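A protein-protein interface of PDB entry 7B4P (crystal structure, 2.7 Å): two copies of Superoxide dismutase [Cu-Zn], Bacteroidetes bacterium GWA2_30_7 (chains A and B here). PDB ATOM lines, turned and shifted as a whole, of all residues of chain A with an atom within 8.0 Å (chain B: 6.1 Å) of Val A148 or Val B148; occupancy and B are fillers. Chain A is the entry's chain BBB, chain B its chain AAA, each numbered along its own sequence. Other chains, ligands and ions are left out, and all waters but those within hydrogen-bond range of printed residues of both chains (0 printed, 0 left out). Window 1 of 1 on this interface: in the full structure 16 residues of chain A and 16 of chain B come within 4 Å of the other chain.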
ATOM      1  N   ALA A   9      19.435  -2.465  13.283  1.00  0.00           N
ATOM      2  CA  ALA A   9      20.146  -1.241  13.726  1.00  0.00           C
ATOM      3  C   ALA A   9      19.165  -0.343  14.485  1.00  0.00           C
ATOM      4  O   ALA A   9      17.982  -0.289  14.088  1.00  0.00           O
ATOM      5  CB  ALA A   9      20.756  -0.526  12.547  1.00  0.00           C
ATOM      6  N   VAL A  10      19.641   0.312  15.548  1.00  0.00           N
ATOM      7  CA  VAL A  10      18.822   1.173  16.452  1.00  0.00           C
ATOM      8  C   VAL A  10      19.522   2.525  16.595  1.00  0.00           C
ATOM      9  O   VAL A  10      20.767   2.541  16.651  1.00  0.00           O
ATOM     10  CB  VAL A  10      18.600   0.511  17.826  1.00  0.00           C
ATOM     11  CG1 VAL A  10      17.668   1.337  18.696  1.00  0.00           C
ATOM     12  CG2 VAL A  10      18.085  -0.912  17.695  1.00  0.00           C
ATOM     13  N   CYS A  11      18.739   3.604  16.651  1.00  0.00           N
ATOM     14  CA  CYS A  11      19.214   5.004  16.798  1.00  0.00           C
ATOM     15  C   CYS A  11      18.229   5.794  17.667  1.00  0.00           C
ATOM     16  O   CYS A  11      17.093   6.026  17.206  1.00  0.00           O
ATOM     17  CB  CYS A  11      19.363   5.682  15.444  1.00  0.00           C
ATOM     18  SG  CYS A  11      19.847   7.423  15.567  1.00  0.00           S
ATOM     19  N   VAL A  12      18.657   6.173  18.877  1.00  0.00           N
ATOM     20  CA  VAL A  12      17.922   7.105  19.781  1.00  0.00           C
ATOM     21  C   VAL A  12      18.365   8.531  19.443  1.00  0.00           C
ATOM     22  O   VAL A  12      19.559   8.836  19.637  1.00  0.00           O
ATOM     23  CB  VAL A  12      18.176   6.779  21.266  1.00  0.00           C
ATOM     24  CG1 VAL A  12      17.373   7.686  22.189  1.00  0.00           C
ATOM     25  CG2 VAL A  12      17.889   5.317  21.574  1.00  0.00           C
ATOM     26  N   ILE A  13      17.448   9.366  18.945  1.00  0.00           N
ATOM     27  CA  ILE A  13      17.722  10.807  18.672  1.00  0.00           C
ATOM     28  C   ILE A  13      17.422  11.600  19.950  1.00  0.00           C
ATOM     29  O   ILE A  13      16.387  11.340  20.592  1.00  0.00           O
ATOM     30  CB  ILE A  13      16.955  11.333  17.436  1.00  0.00           C
ATOM     31  CG1 ILE A  13      15.480  11.627  17.719  1.00  0.00           C
ATOM     32  CG2 ILE A  13      17.113  10.383  16.256  1.00  0.00           C
ATOM     33  CD1 ILE A  13      14.782  12.354  16.592  1.00  0.00           C
ATOM     34  N   TYR A  14      18.338  12.494  20.325  1.00  0.00           N
ATOM     35  CA  TYR A  14      18.192  13.471  21.436  1.00  0.00           C
ATOM     36  C   TYR A  14      18.157  14.865  20.818  1.00  0.00           C
ATOM     37  O   TYR A  14      18.652  15.059  19.709  1.00  0.00           O
ATOM     38  CB  TYR A  14      19.324  13.292  22.448  1.00  0.00           C
ATOM     39  CG  TYR A  14      19.340  11.945  23.125  1.00  0.00           C
ATOM     40  CD1 TYR A  14      18.604  11.718  24.277  1.00  0.00           C
ATOM     41  CD2 TYR A  14      20.081  10.891  22.611  1.00  0.00           C
ATOM     42  CE1 TYR A  14      18.610  10.483  24.907  1.00  0.00           C
ATOM     43  CE2 TYR A  14      20.094   9.649  23.226  1.00  0.00           C
ATOM     44  CZ  TYR A  14      19.356   9.443  24.380  1.00  0.00           C
ATOM     45  OH  TYR A  14      19.370   8.220  24.988  1.00  0.00           O
ATOM     46  N   ILE A  25      14.511   5.184  16.269  1.00  0.00           N
ATOM     47  CA  ILE A  25      14.461   4.735  14.847  1.00  0.00           C
ATOM     48  C   ILE A  25      15.105   3.348  14.776  1.00  0.00           C
ATOM     49  O   ILE A  25      16.247   3.210  15.250  1.00  0.00           O
ATOM     50  CB  ILE A  25      15.177   5.740  13.922  1.00  0.00           C
ATOM     51  CG1 ILE A  25      14.710   7.178  14.168  1.00  0.00           C
ATOM     52  CG2 ILE A  25      15.012   5.338  12.464  1.00  0.00           C
ATOM     53  CD1 ILE A  25      15.661   8.228  13.653  1.00  0.00           C
ATOM     54  N   PHE A  27      16.135   0.091  12.103  1.00  0.00           N
ATOM     55  CA  PHE A  27      16.394  -0.393  10.723  1.00  0.00           C
ATOM     56  C   PHE A  27      16.470  -1.922  10.768  1.00  0.00           C
ATOM     57  O   PHE A  27      17.462  -2.452  11.315  1.00  0.00           O
ATOM     58  CB  PHE A  27      17.686   0.204  10.159  1.00  0.00           C
ATOM     59  CG  PHE A  27      17.819   1.697  10.313  1.00  0.00           C
ATOM     60  CD1 PHE A  27      18.248   2.249  11.511  1.00  0.00           C
ATOM     61  CD2 PHE A  27      17.530   2.549   9.259  1.00  0.00           C
ATOM     62  CE1 PHE A  27      18.374   3.622  11.651  1.00  0.00           C
ATOM     63  CE2 PHE A  27      17.657   3.922   9.402  1.00  0.00           C
ATOM     64  CZ  PHE A  27      18.079   4.455  10.597  1.00  0.00           C
ATOM     65  N   CYS A  55      29.225  11.741   9.716  1.00  0.00           N
ATOM     66  CA  CYS A  55      29.904  11.632  11.037  1.00  0.00           C
ATOM     67  C   CYS A  55      28.877  11.279  12.121  1.00  0.00           C
ATOM     68  O   CYS A  55      27.817  11.936  12.172  1.00  0.00           O
ATOM     69  CB  CYS A  55      30.660  12.909  11.386  1.00  0.00           C
ATOM     70  SG  CYS A  55      32.233  13.065  10.498  1.00  0.00           S
ATOM     71  N   GLY A  56      29.189  10.271  12.945  1.00  0.00           N
ATOM     72  CA  GLY A  56      28.381   9.841  14.103  1.00  0.00           C
ATOM     73  C   GLY A  56      28.772  10.605  15.357  1.00  0.00           C
ATOM     74  O   GLY A  56      29.127   9.956  16.362  1.00  0.00           O
ATOM     75  N   ASP A  57      28.703  11.937  15.295  1.00  0.00           N
ATOM     76  CA  ASP A  57      29.161  12.874  16.354  1.00  0.00           C
ATOM     77  C   ASP A  57      28.022  13.853  16.660  1.00  0.00           C
ATOM     78  O   ASP A  57      27.758  14.734  15.820  1.00  0.00           O
ATOM     79  CB  ASP A  57      30.445  13.580  15.909  1.00  0.00           C
ATOM     80  CG  ASP A  57      31.044  14.528  16.936  1.00  0.00           C
ATOM     81  OD1 ASP A  57      30.331  14.893  17.892  1.00  0.00           O
ATOM     82  OD2 ASP A  57      32.222  14.902  16.763  1.00  0.00           O
ATOM     83  N   CYS A  58      27.367  13.687  17.813  1.00  0.00           N
ATOM     84  CA  CYS A  58      26.256  14.550  18.298  1.00  0.00           C
ATOM     85  C   CYS A  58      26.723  15.358  19.515  1.00  0.00           C
ATOM     86  O   CYS A  58      25.869  15.687  20.362  1.00  0.00           O
ATOM     87  CB  CYS A  58      25.026  13.718  18.646  1.00  0.00           C
ATOM     88  SG  CYS A  58      24.389  12.731  17.265  1.00  0.00           S
ATOM     89  N   SER A  59      28.019  15.684  19.582  1.00  0.00           N
ATOM     90  CA  SER A  59      28.669  16.385  20.722  1.00  0.00           C
ATOM     91  C   SER A  59      28.410  17.895  20.645  1.00  0.00           C
ATOM     92  O   SER A  59      28.496  18.558  21.695  1.00  0.00           O
ATOM     93  CB  SER A  59      30.146  16.082  20.776  1.00  0.00           C
ATOM     94  OG  SER A  59      30.830  16.697  19.697  1.00  0.00           O
ATOM     95  N   ILE A 118      25.570   2.083   7.300  1.00  0.00           N
ATOM     96  CA  ILE A 118      24.981   3.217   8.076  1.00  0.00           C
ATOM     97  C   ILE A 118      25.365   3.076   9.555  1.00  0.00           C
ATOM     98  O   ILE A 118      25.132   4.035  10.318  1.00  0.00           O
ATOM     99  CB  ILE A 118      23.451   3.304   7.886  1.00  0.00           C
ATOM    100  CG1 ILE A 118      22.709   2.117   8.506  1.00  0.00           C
ATOM    101  CG2 ILE A 118      23.105   3.477   6.414  1.00  0.00           C
ATOM    102  CD1 ILE A 118      21.217   2.328   8.614  1.00  0.00           C
ATOM    103  N   ILE A 119      25.927   1.929   9.947  1.00  0.00           N
ATOM    104  CA  ILE A 119      26.362   1.646  11.348  1.00  0.00           C
ATOM    105  C   ILE A 119      27.477   2.635  11.708  1.00  0.00           C
ATOM    106  O   ILE A 119      28.470   2.702  10.958  1.00  0.00           O
ATOM    107  CB  ILE A 119      26.809   0.177  11.503  1.00  0.00           C
ATOM    108  CG1 ILE A 119      25.695  -0.809  11.133  1.00  0.00           C
ATOM    109  CG2 ILE A 119      27.342  -0.081  12.905  1.00  0.00           C
ATOM    110  CD1 ILE A 119      24.401  -0.611  11.904  1.00  0.00           C
ATOM    111  N   GLY A 120      27.295   3.392  12.796  1.00  0.00           N
ATOM    112  CA  GLY A 120      28.267   4.388  13.288  1.00  0.00           C
ATOM    113  C   GLY A 120      28.059   5.757  12.666  1.00  0.00           C
ATOM    114  O   GLY A 120      28.823   6.678  13.008  1.00  0.00           O
ATOM    115  N   ARG A 121      27.076   5.891  11.772  1.00  0.00           N
ATOM    116  CA  ARG A 121      26.662   7.190  11.177  1.00  0.00           C
ATOM    117  C   ARG A 121      25.635   7.835  12.111  1.00  0.00           C
ATOM    118  O   ARG A 121      25.250   7.183  13.099  1.00  0.00           O
ATOM    119  CB  ARG A 121      26.091   6.989   9.769  1.00  0.00           C
ATOM    120  CG  ARG A 121      26.990   6.195   8.830  1.00  0.00           C
ATOM    121  CD  ARG A 121      28.306   6.889   8.549  1.00  0.00           C
ATOM    122  NE  ARG A 121      29.230   6.040   7.811  1.00  0.00           N
ATOM    123  CZ  ARG A 121      30.473   6.379   7.477  1.00  0.00           C
ATOM    124  NH1 ARG A 121      30.956   7.563   7.813  1.00  0.00           N
ATOM    125  NH2 ARG A 121      31.230   5.528   6.807  1.00  0.00           N
ATOM    126  N   SER A 122      25.217   9.065  11.808  1.00  0.00           N
ATOM    127  CA  SER A 122      24.256   9.853  12.620  1.00  0.00           C
ATOM    128  C   SER A 122      22.929  10.007  11.872  1.00  0.00           C
ATOM    129  O   SER A 122      22.955  10.107  10.631  1.00  0.00           O
ATOM    130  CB  SER A 122      24.824  11.200  12.990  1.00  0.00           C
ATOM    131  OG  SER A 122      25.221  11.921  11.835  1.00  0.00           O
ATOM    132  N   MET A 123      21.820   9.999  12.616  1.00  0.00           N
ATOM    133  CA  MET A 123      20.486  10.475  12.164  1.00  0.00           C
ATOM    134  C   MET A 123      20.355  11.946  12.569  1.00  0.00           C
ATOM    135  O   MET A 123      20.719  12.271  13.718  1.00  0.00           O
ATOM    136  CB  MET A 123      19.352   9.677  12.815  1.00  0.00           C
ATOM    137  CG  MET A 123      19.181   8.261  12.277  1.00  0.00           C
ATOM    138  SD  MET A 123      18.682   8.195  10.532  1.00  0.00           S
ATOM    139  CE  MET A 123      17.378   9.422  10.486  1.00  0.00           C
ATOM    140  N   ILE A 124      19.877  12.795  11.655  1.00  0.00           N
ATOM    141  CA  ILE A 124      19.604  14.242  11.903  1.00  0.00           C
ATOM    142  C   ILE A 124      18.164  14.546  11.472  1.00  0.00           C
ATOM    143  O   ILE A 124      17.802  14.215  10.323  1.00  0.00           O
ATOM    144  CB  ILE A 124      20.622  15.137  11.164  1.00  0.00           C
ATOM    145  CG1 ILE A 124      22.031  15.007  11.754  1.00  0.00           C
ATOM    146  CG2 ILE A 124      20.159  16.588  11.133  1.00  0.00           C
ATOM    147  CD1 ILE A 124      22.191  15.624  13.127  1.00  0.00           C
ATOM    148  N   CYS A 146      19.751  14.956  16.975  1.00  0.00           N
ATOM    149  CA  CYS A 146      20.906  14.137  16.517  1.00  0.00           C
ATOM    150  C   CYS A 146      20.887  12.792  17.251  1.00  0.00           C
ATOM    151  O   CYS A 146      20.420  12.751  18.405  1.00  0.00           O
ATOM    152  CB  CYS A 146      22.228  14.850  16.782  1.00  0.00           C
ATOM    153  SG  CYS A 146      23.652  14.099  15.947  1.00  0.00           S
ATOM    154  N   GLY A 147      21.383  11.740  16.597  1.00  0.00           N
ATOM    155  CA  GLY A 147      21.542  10.395  17.181  1.00  0.00           C
ATOM    156  C   GLY A 147      22.494   9.555  16.352  1.00  0.00           C
ATOM    157  O   GLY A 147      22.577   9.801  15.139  1.00  0.00           O
ATOM    158  N   VAL A 148      23.187   8.605  16.985  1.00  0.00           N
ATOM    159  CA  VAL A 148      24.150   7.676  16.323  1.00  0.00           C
ATOM    160  C   VAL A 148      23.457   6.325  16.112  1.00  0.00           C
ATOM    161  O   VAL A 148      22.783   5.845  17.046  1.00  0.00           O
ATOM    162  CB  VAL A 148      25.451   7.535  17.140  1.00  0.00           C
ATOM    163  CG1 VAL A 148      26.431   6.563  16.499  1.00  0.00           C
ATOM    164  CG2 VAL A 148      26.117   8.885  17.366  1.00  0.00           C
ATOM    165  N   ILE A 149      23.625   5.747  14.919  1.00  0.00           N
ATOM    166  CA  ILE A 149      23.069   4.420  14.521  1.00  0.00           C
ATOM    167  C   ILE A 149      23.996   3.335  15.075  1.00  0.00           C
ATOM    168  O   ILE A 149      25.190   3.346  14.718  1.00  0.00           O
ATOM    169  CB  ILE A 149      22.915   4.327  12.988  1.00  0.00           C
ATOM    170  CG1 ILE A 149      22.013   5.437  12.439  1.00  0.00           C
ATOM    171  CG2 ILE A 149      22.420   2.947  12.573  1.00  0.00           C
ATOM    172  CD1 ILE A 149      22.181   5.691  10.960  1.00  0.00           C
ATOM    173  N   GLY A 150      23.462   2.444  15.915  1.00  0.00           N
ATOM    174  CA  GLY A 150      24.209   1.337  16.543  1.00  0.00           C
ATOM    175  C   GLY A 150      23.716  -0.024  16.079  1.00  0.00           C
ATOM    176  O   GLY A 150      22.635  -0.088  15.461  1.00  0.00           O
ATOM    177  N   ILE A 151      24.485  -1.072  16.378  1.00  0.00           N
ATOM    178  CA  ILE A 151      24.169  -2.489  16.030  1.00  0.00           C
ATOM    179  C   ILE A 151      23.090  -3.000  16.996  1.00  0.00           C
ATOM    180  O   ILE A 151      23.273  -2.838  18.218  1.00  0.00           O
ATOM    181  CB  ILE A 151      25.443  -3.359  16.075  1.00  0.00           C
ATOM    182  CG1 ILE A 151      26.496  -2.872  15.074  1.00  0.00           C
ATOM    183  CG2 ILE A 151      25.103  -4.828  15.865  1.00  0.00           C
ATOM    184  CD1 ILE A 151      27.901  -3.328  15.384  1.00  0.00           C
ATOM    185  N   VAL B  10      33.512   8.983  18.273  1.00  0.00           N
ATOM    186  CA  VAL B  10      32.866   9.883  19.275  1.00  0.00           C
ATOM    187  C   VAL B  10      31.628   9.175  19.832  1.00  0.00           C
ATOM    188  O   VAL B  10      30.944   8.480  19.057  1.00  0.00           O
ATOM    189  CB  VAL B  10      32.501  11.248  18.662  1.00  0.00           C
ATOM    190  CG1 VAL B  10      31.925  12.197  19.704  1.00  0.00           C
ATOM    191  CG2 VAL B  10      33.689  11.885  17.958  1.00  0.00           C
ATOM    192  N   CYS B  11      31.369   9.356  21.129  1.00  0.00           N
ATOM    193  CA  CYS B  11      30.215   8.775  21.865  1.00  0.00           C
ATOM    194  C   CYS B  11      29.721   9.772  22.919  1.00  0.00           C
ATOM    195  O   CYS B  11      30.465  10.022  23.887  1.00  0.00           O
ATOM    196  CB  CYS B  11      30.599   7.461  22.535  1.00  0.00           C
ATOM    197  SG  CYS B  11      29.259   6.754  23.527  1.00  0.00           S
ATOM    198  N   VAL B  12      28.522  10.323  22.719  1.00  0.00           N
ATOM    199  CA  VAL B  12      27.798  11.164  23.717  1.00  0.00           C
ATOM    200  C   VAL B  12      26.951  10.230  24.586  1.00  0.00           C
ATOM    201  O   VAL B  12      26.023   9.601  24.035  1.00  0.00           O
ATOM    202  CB  VAL B  12      26.923  12.236  23.039  1.00  0.00           C
ATOM    203  CG1 VAL B  12      26.266  13.146  24.065  1.00  0.00           C
ATOM    204  CG2 VAL B  12      27.704  13.052  22.023  1.00  0.00           C
ATOM    205  N   GLY B  56      24.416  -1.544  20.325  1.00  0.00           N
ATOM    206  CA  GLY B  56      24.359  -0.068  20.289  1.00  0.00           C
ATOM    207  C   GLY B  56      22.929   0.434  20.400  1.00  0.00           C
ATOM    208  O   GLY B  56      22.487   1.180  19.499  1.00  0.00           O
ATOM    209  N   ASP B  57      22.235   0.037  21.469  1.00  0.00           N
ATOM    210  CA  ASP B  57      20.788   0.296  21.696  1.00  0.00           C
ATOM    211  C   ASP B  57      20.618   0.902  23.095  1.00  0.00           C
ATOM    212  O   ASP B  57      20.769   0.157  24.081  1.00  0.00           O
ATOM    213  CB  ASP B  57      19.983  -0.994  21.506  1.00  0.00           C
ATOM    214  CG  ASP B  57      18.479  -0.841  21.659  1.00  0.00           C
ATOM    215  OD1 ASP B  57      18.040   0.189  22.207  1.00  0.00           O
ATOM    216  OD2 ASP B  57      17.756  -1.762  21.233  1.00  0.00           O
ATOM    217  N   CYS B  58      20.328   2.205  23.167  1.00  0.00           N
ATOM    218  CA  CYS B  58      20.102   2.961  24.427  1.00  0.00           C
ATOM    219  C   CYS B  58      18.626   3.370  24.534  1.00  0.00           C
ATOM    220  O   CYS B  58      18.347   4.408  25.166  1.00  0.00           O
ATOM    221  CB  CYS B  58      21.002   4.192  24.490  1.00  0.00           C
ATOM    222  SG  CYS B  58      22.772   3.810  24.397  1.00  0.00           S
ATOM    223  N   GLY B 120      29.497   1.504  16.336  1.00  0.00           N
ATOM    224  CA  GLY B 120      28.108   1.010  16.387  1.00  0.00           C
ATOM    225  C   GLY B 120      27.812   0.245  17.666  1.00  0.00           C
ATOM    226  O   GLY B 120      26.665  -0.219  17.823  1.00  0.00           O
ATOM    227  N   ARG B 121      28.805   0.107  18.550  1.00  0.00           N
ATOM    228  CA  ARG B 121      28.638  -0.486  19.902  1.00  0.00           C
ATOM    229  C   ARG B 121      28.202   0.629  20.857  1.00  0.00           C
ATOM    230  O   ARG B 121      28.168   1.796  20.422  1.00  0.00           O
ATOM    231  CB  ARG B 121      29.934  -1.155  20.370  1.00  0.00           C
ATOM    232  CG  ARG B 121      30.522  -2.154  19.382  1.00  0.00           C
ATOM    233  CD  ARG B 121      29.614  -3.341  19.133  1.00  0.00           C
ATOM    234  NE  ARG B 121      30.092  -4.186  18.049  1.00  0.00           N
ATOM    235  CZ  ARG B 121      29.466  -5.269  17.595  1.00  0.00           C
ATOM    236  NH1 ARG B 121      28.320  -5.657  18.132  1.00  0.00           N
ATOM    237  NH2 ARG B 121      29.993  -5.962  16.601  1.00  0.00           N
ATOM    238  N   SER B 122      27.889   0.280  22.107  1.00  0.00           N
ATOM    239  CA  SER B 122      27.418   1.223  23.154  1.00  0.00           C
ATOM    240  C   SER B 122      28.486   1.387  24.241  1.00  0.00           C
ATOM    241  O   SER B 122      29.193   0.408  24.530  1.00  0.00           O
ATOM    242  CB  SER B 122      26.110   0.770  23.748  1.00  0.00           C
ATOM    243  OG  SER B 122      26.212  -0.548  24.264  1.00  0.00           O
ATOM    244  N   MET B 123      28.595   2.599  24.792  1.00  0.00           N
ATOM    245  CA  MET B 123      29.291   2.897  26.071  1.00  0.00           C
ATOM    246  C   MET B 123      28.249   2.838  27.192  1.00  0.00           C
ATOM    247  O   MET B 123      27.154   3.397  26.998  1.00  0.00           O
ATOM    248  CB  MET B 123      29.933   4.290  26.055  1.00  0.00           C
ATOM    249  CG  MET B 123      31.180   4.402  25.186  1.00  0.00           C
ATOM    250  SD  MET B 123      32.573   3.390  25.764  1.00  0.00           S
ATOM    251  CE  MET B 123      32.570   3.763  27.517  1.00  0.00           C
ATOM    252  N   CYS B 146      24.052   5.629  29.043  1.00  0.00           N
ATOM    253  CA  CYS B 146      24.225   4.857  27.782  1.00  0.00           C
ATOM    254  C   CYS B 146      24.561   5.823  26.641  1.00  0.00           C
ATOM    255  O   CYS B 146      24.104   6.977  26.690  1.00  0.00           O
ATOM    256  CB  CYS B 146      22.958   4.076  27.444  1.00  0.00           C
ATOM    257  SG  CYS B 146      23.185   2.836  26.142  1.00  0.00           S
ATOM    258  N   GLY B 147      25.323   5.356  25.652  1.00  0.00           N
ATOM    259  CA  GLY B 147      25.651   6.104  24.423  1.00  0.00           C
ATOM    260  C   GLY B 147      26.161   5.166  23.343  1.00  0.00           C
ATOM    261  O   GLY B 147      26.734   4.122  23.701  1.00  0.00           O
ATOM    262  N   VAL B 148      25.958   5.519  22.071  1.00  0.00           N
ATOM    263  CA  VAL B 148      26.417   4.727  20.890  1.00  0.00           C
ATOM    264  C   VAL B 148      27.693   5.372  20.337  1.00  0.00           C
ATOM    265  O   VAL B 148      27.734   6.615  20.221  1.00  0.00           O
ATOM    266  CB  VAL B 148      25.313   4.625  19.817  1.00  0.00           C
ATOM    267  CG1 VAL B 148      25.773   3.853  18.590  1.00  0.00           C
ATOM    268  CG2 VAL B 148      24.041   4.008  20.379  1.00  0.00           C
ATOM    269  N   ILE B 149      28.692   4.546  20.012  1.00  0.00           N
ATOM    270  CA  ILE B 149      29.999   4.966  19.429  1.00  0.00           C
ATOM    271  C   ILE B 149      29.801   5.169  17.923  1.00  0.00           C
ATOM    272  O   ILE B 149      29.400   4.204  17.250  1.00  0.00           O
ATOM    273  CB  ILE B 149      31.097   3.924  19.734  1.00  0.00           C
ATOM    274  CG1 ILE B 149      31.268   3.711  21.241  1.00  0.00           C
ATOM    275  CG2 ILE B 149      32.413   4.306  19.072  1.00  0.00           C
ATOM    276  CD1 ILE B 149      31.972   2.425  21.608  1.00  0.00           C
ATOM    277  N   GLY B 150      30.067   6.381  17.429  1.00  0.00           N
ATOM    278  CA  GLY B 150      29.926   6.750  16.007  1.00  0.00           C
ATOM    279  C   GLY B 150      31.261   7.104  15.374  1.00  0.00           C
ATOM    280  O   GLY B 150      32.247   7.284  16.120  1.00  0.00           O
ATOM    281  N   ILE B 151      31.289   7.201  14.043  1.00  0.00           N
ATOM    282  CA  ILE B 151      32.505   7.532  13.240  1.00  0.00           C
ATOM    283  C   ILE B 151      32.766   9.039  13.356  1.00  0.00           C
ATOM    284  O   ILE B 151      31.822   9.817  13.120  1.00  0.00           O
ATOM    285  CB  ILE B 151      32.329   7.080  11.775  1.00  0.00           C
ATOM    286  CG1 ILE B 151      32.113   5.569  11.667  1.00  0.00           C
ATOM    287  CG2 ILE B 151      33.503   7.540  10.925  1.00  0.00           C
ATOM    288  CD1 ILE B 151      31.424   5.138  10.398  1.00  0.00           C
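O of Ile A151 lies within hydrogen-bond range of N of Gly B56, 2.7 Å away. N of Ile A151 is in hydrogen-bond range of O of Gly B120, at 2.8 Å. The backbone carbonyl oxygen of Ile B151 sits at hydrogen-bond distance from the backbone NH of Gly A56 (2.7 Å). The backbone NH of Ile B151 lies within hydrogen-bond range of the backbone carbonyl oxygen of Gly A120.
SG of Cys B11 lies within hydrogen-bond range of O of Val B148 (3.6 Å). The side-chain sulfur (SG) of Cys B58 forms a disulfide with the side-chain sulfur (SG) of Cys B146 (2.0 Å). The backbone NH of Gly B147 is in hydrogen-bond range of the side-chain sulfur of Cys B58 (3.2 Å). O of Val A10 sits at hydrogen-bond distance from N of Gly A150. The side-chain sulfur (SG) of Cys A11 is in hydrogen-bond range of the backbone carbonyl oxygen (O) of Val A148. The side-chain hydroxyl (OG) of Ser A122 lies within hydrogen-bond range of the backbone carbonyl oxygen (O) of Cys A55 (2.6 Å).
Among the printed residues, merely in contact across the chains: Val A10 with Gly B56, Val A10 with Asp B57, Val A12 with Cys B58, Tyr A14 with Cys B58, Cys A55 with Ile B151, Gly A56 with Val B10, Gly A56 with Gly B150, Asp A57 with Val B10, Cys A58 with Val B12, Ser A59 with Val B12, Ile A119 with Gly B120, Ile A119 with Ile B151, Gly A120 with Gly B150, Arg A121 with Ile B151, Val A148 with Val B148, Val A148 with Ile B149, Val A148 with Gly B150, Ile A149 with Val B148, Gly A150 with Gly B56, Gly A150 with Gly B120, Gly A150 with Val B148 and Ile A151 with Arg B121.
Val B148 touches just these residues of chain A: Val A148, Ile A149 and Gly A150. No residue of chain A comes within 4 Å of Gly B147. Printed residues of chain A within 4 Å of Gly B120: Ile A119 (3.7 Å), Gly A150 (3.2 Å) and Ile A151 (2.8 Å). Printed residues of chain B within 4 Å of Ile A149: Val B148 (3.9 Å). Of the printed residues of chain B, Ser A59 touches Val B12. Printed residues of chain A within 4 Å of Arg B121: Ile A151. Of the printed residues of chain B, Ile A151 touches Gly B56, Gly B120 and Arg B121. Cys B11 touches none of the printed residues of chain A. The nearest residue of chain B that does not touch Val A148 is Val B10 (5.1 Å).
Of the 16 printed residues of chain B, 11 touch a printed residue of chain A. Printed residues of chain B that touch a printed residue of chain A: Val B10, Val B12, Gly B56, Asp B57, Cys B58, Gly B120, Arg B121, Val B148, Ile B149, Gly B150 and Ile B151. Hydrophobic or aromatic side chains of chain A within 4 Å of the printed part of chain B: Val A10, Val A12, Tyr A14, Ile A119, Val A148 and Ile A151. Among the printed residues, 26 pairs touch across the chains.
Val A10 touches Gly B56, and with the chains exchanged Gly A56 touches Val B10. Gly A120 touches Gly B150, and with the chains exchanged Gly A150 touches Gly B120. Val B148 touches its own counterpart, Val A148. Val A148 touches Gly B150, and with the chains exchanged Gly A150 touches Val B148. 16 positions are printed for both chains. Of the 26 pairs that touch across the chains among the printed residues, 21 have their exchanged pair printed and touching as well.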
